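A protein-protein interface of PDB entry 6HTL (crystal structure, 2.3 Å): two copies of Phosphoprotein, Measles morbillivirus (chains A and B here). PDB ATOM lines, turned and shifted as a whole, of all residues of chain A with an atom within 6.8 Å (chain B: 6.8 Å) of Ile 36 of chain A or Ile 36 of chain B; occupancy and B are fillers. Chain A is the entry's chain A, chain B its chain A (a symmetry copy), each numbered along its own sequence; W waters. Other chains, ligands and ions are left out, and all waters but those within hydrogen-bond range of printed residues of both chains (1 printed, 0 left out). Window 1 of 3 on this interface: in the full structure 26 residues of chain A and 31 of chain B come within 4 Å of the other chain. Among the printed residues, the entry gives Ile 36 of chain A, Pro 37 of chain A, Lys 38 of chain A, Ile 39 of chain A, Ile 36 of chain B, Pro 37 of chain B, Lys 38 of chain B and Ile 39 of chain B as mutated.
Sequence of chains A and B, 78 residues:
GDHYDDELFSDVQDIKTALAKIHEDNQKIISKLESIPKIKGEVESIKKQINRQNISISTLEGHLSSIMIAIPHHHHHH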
ATOM      1  N   LYS A  32       5.001  28.072 -16.668  1.00  0.00           N
ATOM      2  CA  LYS A  32       6.433  28.013 -16.367  1.00  0.00           C
ATOM      3  C   LYS A  32       6.799  26.701 -15.687  1.00  0.00           C
ATOM      4  O   LYS A  32       7.940  26.244 -15.816  1.00  0.00           O
ATOM      5  CB  LYS A  32       6.868  29.218 -15.522  1.00  0.00           C
ATOM      6  CG  LYS A  32       6.762  30.530 -16.279  1.00  0.00           C
ATOM      7  CD  LYS A  32       7.189  31.725 -15.452  1.00  0.00           C
ATOM      8  CE  LYS A  32       7.043  32.986 -16.262  1.00  0.00           C
ATOM      9  NZ  LYS A  32       8.046  33.060 -17.368  1.00  0.00           N
ATOM     10  N   LEU A  33       5.816  26.078 -15.001  1.00  0.00           N
ATOM     11  CA  LEU A  33       5.943  24.797 -14.311  1.00  0.00           C
ATOM     12  C   LEU A  33       5.727  23.577 -15.243  1.00  0.00           C
ATOM     13  O   LEU A  33       5.843  22.434 -14.796  1.00  0.00           O
ATOM     14  CB  LEU A  33       4.988  24.737 -13.112  1.00  0.00           C
ATOM     15  CG  LEU A  33       5.297  25.632 -11.911  1.00  0.00           C
ATOM     16  CD1 LEU A  33       4.132  25.628 -10.924  1.00  0.00           C
ATOM     17  CD2 LEU A  33       6.574  25.204 -11.217  1.00  0.00           C
ATOM     18  N   GLU A  34       5.444  23.815 -16.532  1.00  0.00           N
ATOM     19  CA  GLU A  34       5.243  22.742 -17.514  1.00  0.00           C
ATOM     20  C   GLU A  34       6.523  21.964 -17.786  1.00  0.00           C
ATOM     21  O   GLU A  34       6.443  20.787 -18.117  1.00  0.00           O
ATOM     22  CB  GLU A  34       4.697  23.280 -18.853  1.00  0.00           C
ATOM     23  CG  GLU A  34       3.298  23.877 -18.787  1.00  0.00           C
ATOM     24  CD  GLU A  34       2.187  22.990 -19.298  1.00  0.00           C
ATOM     25  OE1 GLU A  34       2.207  22.644 -20.502  1.00  0.00           O
ATOM     26  OE2 GLU A  34       1.285  22.655 -18.499  1.00  0.00           O
ATOM     27  N   SER A  35       7.695  22.603 -17.659  1.00  0.00           N
ATOM     28  CA  SER A  35       8.937  21.919 -17.961  1.00  0.00           C
ATOM     29  C   SER A  35       9.558  21.173 -16.756  1.00  0.00           C
ATOM     30  O   SER A  35      10.583  20.497 -16.938  1.00  0.00           O
ATOM     31  CB  SER A  35       9.929  22.865 -18.629  1.00  0.00           C
ATOM     32  OG  SER A  35      10.438  23.824 -17.725  1.00  0.00           O
ATOM     33  N   ILE A  36       8.906  21.218 -15.561  1.00  0.00           N
ATOM     34  CA  ILE A  36       9.380  20.503 -14.364  1.00  0.00           C
ATOM     35  C   ILE A  36       9.360  18.962 -14.625  1.00  0.00           C
ATOM     36  O   ILE A  36      10.389  18.323 -14.399  1.00  0.00           O
ATOM     37  CB  ILE A  36       8.674  20.951 -13.029  1.00  0.00           C
ATOM     38  CG1 ILE A  36       9.308  22.232 -12.433  1.00  0.00           C
ATOM     39  CG2 ILE A  36       8.772  19.881 -11.958  1.00  0.00           C
ATOM     40  CD1 ILE A  36       9.148  23.476 -13.142  1.00  0.00           C
ATOM     41  N   PRO A  37       8.279  18.355 -15.185  1.00  0.00           N
ATOM     42  CA  PRO A  37       8.322  16.908 -15.450  1.00  0.00           C
ATOM     43  C   PRO A  37       9.296  16.506 -16.568  1.00  0.00           C
ATOM     44  O   PRO A  37       9.678  15.341 -16.645  1.00  0.00           O
ATOM     45  CB  PRO A  37       6.869  16.570 -15.806  1.00  0.00           C
ATOM     46  CG  PRO A  37       6.061  17.732 -15.368  1.00  0.00           C
ATOM     47  CD  PRO A  37       6.952  18.906 -15.528  1.00  0.00           C
ATOM     48  N   LYS A  38       9.691  17.469 -17.436  1.00  0.00           N
ATOM     49  CA  LYS A  38      10.660  17.235 -18.508  1.00  0.00           C
ATOM     50  C   LYS A  38      12.041  17.106 -17.852  1.00  0.00           C
ATOM     51  O   LYS A  38      12.767  16.155 -18.133  1.00  0.00           O
ATOM     52  CB  LYS A  38      10.643  18.393 -19.540  1.00  0.00           C
ATOM     53  CG  LYS A  38       9.324  18.546 -20.292  1.00  0.00           C
ATOM     54  CD  LYS A  38       9.258  19.848 -21.090  1.00  0.00           C
ATOM     55  CE  LYS A  38       7.975  19.970 -21.883  1.00  0.00           C
ATOM     56  NZ  LYS A  38       7.603  21.390 -22.137  1.00  0.00           N
ATOM     57  N   ILE A  39      12.358  18.039 -16.930  1.00  0.00           N
ATOM     58  CA  ILE A  39      13.599  18.096 -16.163  1.00  0.00           C
ATOM     59  C   ILE A  39      13.770  16.843 -15.323  1.00  0.00           C
ATOM     60  O   ILE A  39      14.856  16.258 -15.360  1.00  0.00           O
ATOM     61  CB  ILE A  39      13.714  19.386 -15.309  1.00  0.00           C
ATOM     62  CG1 ILE A  39      13.717  20.639 -16.200  1.00  0.00           C
ATOM     63  CG2 ILE A  39      14.966  19.355 -14.404  1.00  0.00           C
ATOM     64  CD1 ILE A  39      13.288  21.968 -15.446  1.00  0.00           C
ATOM     65  N   LYS A  40      12.716  16.427 -14.579  1.00  0.00           N
ATOM     66  CA  LYS A  40      12.772  15.219 -13.738  1.00  0.00           C
ATOM     67  C   LYS A  40      13.115  13.977 -14.587  1.00  0.00           C
ATOM     68  O   LYS A  40      14.002  13.218 -14.225  1.00  0.00           O
ATOM     69  CB  LYS A  40      11.470  15.025 -12.942  1.00  0.00           C
ATOM     70  CG  LYS A  40      11.579  13.969 -11.846  1.00  0.00           C
ATOM     71  CD  LYS A  40      10.210  13.572 -11.331  1.00  0.00           C
ATOM     72  CE  LYS A  40      10.108  12.083 -11.120  1.00  0.00           C
ATOM     73  NZ  LYS A  40       8.837  11.709 -10.454  1.00  0.00           N
ATOM     74  N   GLY A  41      12.452  13.850 -15.734  1.00  0.00           N
ATOM     75  CA  GLY A  41      12.640  12.771 -16.686  1.00  0.00           C
ATOM     76  C   GLY A  41      14.041  12.725 -17.234  1.00  0.00           C
ATOM     77  O   GLY A  41      14.657  11.658 -17.233  1.00  0.00           O
ATOM     78  N   LYS B  32       2.501  20.447  -8.687  1.00  0.00           N
ATOM     79  CA  LYS B  32       3.531  20.491  -9.727  1.00  0.00           C
ATOM     80  C   LYS B  32       4.916  20.678  -9.123  1.00  0.00           C
ATOM     81  O   LYS B  32       5.907  20.242  -9.721  1.00  0.00           O
ATOM     82  CB  LYS B  32       3.223  21.582 -10.760  1.00  0.00           C
ATOM     83  CG  LYS B  32       1.974  21.283 -11.571  1.00  0.00           C
ATOM     84  CD  LYS B  32       1.662  22.356 -12.593  1.00  0.00           C
ATOM     85  CE  LYS B  32       0.407  21.997 -13.344  1.00  0.00           C
ATOM     86  NZ  LYS B  32       0.611  20.825 -14.248  1.00  0.00           N
ATOM     87  N   LEU B  33       4.976  21.287  -7.919  1.00  0.00           N
ATOM     88  CA  LEU B  33       6.194  21.529  -7.150  1.00  0.00           C
ATOM     89  C   LEU B  33       6.620  20.317  -6.282  1.00  0.00           C
ATOM     90  O   LEU B  33       7.652  20.374  -5.612  1.00  0.00           O
ATOM     91  CB  LEU B  33       6.040  22.786  -6.285  1.00  0.00           C
ATOM     92  CG  LEU B  33       5.992  24.139  -6.997  1.00  0.00           C
ATOM     93  CD1 LEU B  33       5.598  25.245  -6.022  1.00  0.00           C
ATOM     94  CD2 LEU B  33       7.318  24.465  -7.654  1.00  0.00           C
ATOM     95  N   GLU B  34       5.849  19.220  -6.316  1.00  0.00           N
ATOM     96  CA  GLU B  34       6.163  18.003  -5.556  1.00  0.00           C
ATOM     97  C   GLU B  34       7.422  17.315  -6.068  1.00  0.00           C
ATOM     98  O   GLU B  34       8.099  16.660  -5.285  1.00  0.00           O
ATOM     99  CB  GLU B  34       4.999  16.991  -5.582  1.00  0.00           C
ATOM    100  CG  GLU B  34       3.730  17.449  -4.879  1.00  0.00           C
ATOM    101  CD  GLU B  34       3.502  16.872  -3.502  1.00  0.00           C
ATOM    102  OE1 GLU B  34       3.363  15.632  -3.391  1.00  0.00           O
ATOM    103  OE2 GLU B  34       3.444  17.662  -2.534  1.00  0.00           O
ATOM    104  N   SER B  35       7.736  17.446  -7.365  1.00  0.00           N
ATOM    105  CA  SER B  35       8.892  16.764  -7.909  1.00  0.00           C
ATOM    106  C   SER B  35      10.207  17.576  -7.820  1.00  0.00           C
ATOM    107  O   SER B  35      11.263  17.043  -8.193  1.00  0.00           O
ATOM    108  CB  SER B  35       8.615  16.268  -9.324  1.00  0.00           C
ATOM    109  OG  SER B  35       8.547  17.329 -10.254  1.00  0.00           O
ATOM    110  N   ILE B  36      10.165  18.814  -7.255  1.00  0.00           N
ATOM    111  CA  ILE B  36      11.363  19.651  -7.072  1.00  0.00           C
ATOM    112  C   ILE B  36      12.361  18.943  -6.099  1.00  0.00           C
ATOM    113  O   ILE B  36      13.528  18.803  -6.468  1.00  0.00           O
ATOM    114  CB  ILE B  36      11.047  21.151  -6.710  1.00  0.00           C
ATOM    115  CG1 ILE B  36      10.726  22.001  -7.964  1.00  0.00           C
ATOM    116  CG2 ILE B  36      12.223  21.820  -6.023  1.00  0.00           C
ATOM    117  CD1 ILE B  36       9.508  21.735  -8.686  1.00  0.00           C
ATOM    118  N   PRO B  37      11.937  18.400  -4.926  1.00  0.00           N
ATOM    119  CA  PRO B  37      12.905  17.706  -4.061  1.00  0.00           C
ATOM    120  C   PRO B  37      13.426  16.383  -4.642  1.00  0.00           C
ATOM    121  O   PRO B  37      14.467  15.900  -4.203  1.00  0.00           O
ATOM    122  CB  PRO B  37      12.128  17.494  -2.757  1.00  0.00           C
ATOM    123  CG  PRO B  37      10.944  18.382  -2.839  1.00  0.00           C
ATOM    124  CD  PRO B  37      10.609  18.449  -4.282  1.00  0.00           C
ATOM    125  N   LYS B  38      12.699  15.796  -5.624  1.00  0.00           N
ATOM    126  CA  LYS B  38      13.113  14.568  -6.304  1.00  0.00           C
ATOM    127  C   LYS B  38      14.278  14.933  -7.233  1.00  0.00           C
ATOM    128  O   LYS B  38      15.312  14.269  -7.210  1.00  0.00           O
ATOM    129  CB  LYS B  38      11.938  13.949  -7.106  1.00  0.00           C
ATOM    130  CG  LYS B  38      10.762  13.492  -6.247  1.00  0.00           C
ATOM    131  CD  LYS B  38       9.532  13.145  -7.085  1.00  0.00           C
ATOM    132  CE  LYS B  38       8.387  12.634  -6.237  1.00  0.00           C
ATOM    133  NZ  LYS B  38       7.062  12.881  -6.871  1.00  0.00           N
ATOM    134  N   ILE B  39      14.115  16.033  -7.997  1.00  0.00           N
ATOM    135  CA  ILE B  39      15.098  16.580  -8.929  1.00  0.00           C
ATOM    136  C   ILE B  39      16.374  16.965  -8.200  1.00  0.00           C
ATOM    137  O   ILE B  39      17.451  16.586  -8.666  1.00  0.00           O
ATOM    138  CB  ILE B  39      14.534  17.755  -9.770  1.00  0.00           C
ATOM    139  CG1 ILE B  39      13.350  17.296 -10.636  1.00  0.00           C
ATOM    140  CG2 ILE B  39      15.632  18.404 -10.643  1.00  0.00           C
ATOM    141  CD1 ILE B  39      12.388  18.472 -11.091  1.00  0.00           C
ATOM    142  N   LYS B  40      16.262  17.702  -7.067  1.00  0.00           N
ATOM    143  CA  LYS B  40      17.433  18.119  -6.279  1.00  0.00           C
ATOM    144  C   LYS B  40      18.249  16.892  -5.820  1.00  0.00           C
ATOM    145  O   LYS B  40      19.459  16.867  -5.992  1.00  0.00           O
ATOM    146  CB  LYS B  40      17.026  19.011  -5.093  1.00  0.00           C
ATOM    147  CG  LYS B  40      18.207  19.706  -4.422  1.00  0.00           C
ATOM    148  CD  LYS B  40      17.811  20.282  -3.077  1.00  0.00           C
ATOM    149  CE  LYS B  40      18.876  20.047  -2.038  1.00  0.00           C
ATOM    150  NZ  LYS B  40      18.573  20.756  -0.771  1.00  0.00           N
ATOM    151  N   GLY B  41      17.549  15.878  -5.319  1.00  0.00           N
ATOM    152  CA  GLY B  41      18.119  14.627  -4.852  1.00  0.00           C
ATOM    153  C   GLY B  41      18.840  13.881  -5.943  1.00  0.00           C
ATOM    154  O   GLY B  41      19.982  13.465  -5.740  1.00  0.00           O
HETATM  155  O   HOH W   1       2.111  22.785 -15.942  1.00  0.00           O
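Water W1 bridges OE2 of Glu 34 of chain A (2.7 Å) and NZ of Lys 32 of chain B (3.0 Å).
Ile 36 of chain A touches Lys 32 of chain B, but with the chains exchanged Lys 32 of chain A does not touch Ile 36 of chain B (8.6 Å).
Ile 36 of chain A touches Ile 39 of chain B, but with the chains exchanged Ile 39 of chain A does not touch Ile 36 of chain B (7.7 Å).
Ile 39 of chain B touches its own counterpart, Ile 39 of chain A.
Lys 40 of chain A touches Ser 35 of chain B, but with the chains exchanged Ser 35 of chain A does not touch Lys 40 of chain B (11.7 Å).
Of the 9 pairs that touch across the chains among the printed residues, 3 have their exchanged pair printed and touching as well.
Of the 10 printed residues of chain A, 4 touch a printed residue of chain B.
Hydrophobic or aromatic side chains of chain A within 4 Å of the printed part of chain B: Leu 33, Ile 36 and Ile 39.
Of the 10 printed residues of chain B, 6 touch a printed residue of chain A.
Hydrophobic or aromatic side chains of chain B that line the printed part of chain A: Leu 33, Ile 36 and Ile 39.
Among the printed residues, no Asp or Glu carboxylate lies within 4 Å of a Lys or Arg side-chain nitrogen of the other chain.
Among the printed residues, pairs that only touch across the chains: Leu 33 of chain A with Leu 33 of chain B (3.7 Å), Ile 36 of chain A with Lys 32 of chain B (3.7 Å), Ile 36 of chain A with Ser 35 of chain B (3.1 Å), Ile 36 of chain A with Ile 36 of chain B (3.8 Å), Ile 36 of chain A with Ile 39 of chain B (3.9 Å), Ile 39 of chain A with Ile 39 of chain B (3.9 Å), Lys 40 of chain A with Ser 35 of chain B (3.7 Å), Lys 40 of chain A with Lys 38 of chain B (3.7 Å) and Lys 40 of chain A with Ile 39 of chain B (3.7 Å).
Of chain B, only Lys 32, Ser 35, Ile 36 and Ile 39 come within 4 Å of Ile 36 of chain A.
Lys 38 of chain A touches none of the printed residues of chain B.
Of the printed residues of chain B, Ile 39 of chain A touches Ile 39 (3.9 Å).
Printed residues of chain B within 4 Å of Lys 40 of chain A: Ser 35, Lys 38 and Ile 39.
Of the printed residues of chain A, Ile 36 of chain B touches Ile 36 (3.8 Å).
Of the printed residues of chain A, Ile 39 of chain B touches Ile 36, Ile 39 and Lys 40.
The nearest residue of chain B that does not touch Ile 36 of chain A is Leu 33 of chain B (5.6 Å).
The nearest residue of chain A that does not touch Ile 36 of chain B is Leu 33 of chain A (5.2 Å).
The nearest printed residue of chain A that does not touch Leu 33 of chain B is Ile 36 of chain A (5.6 Å).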
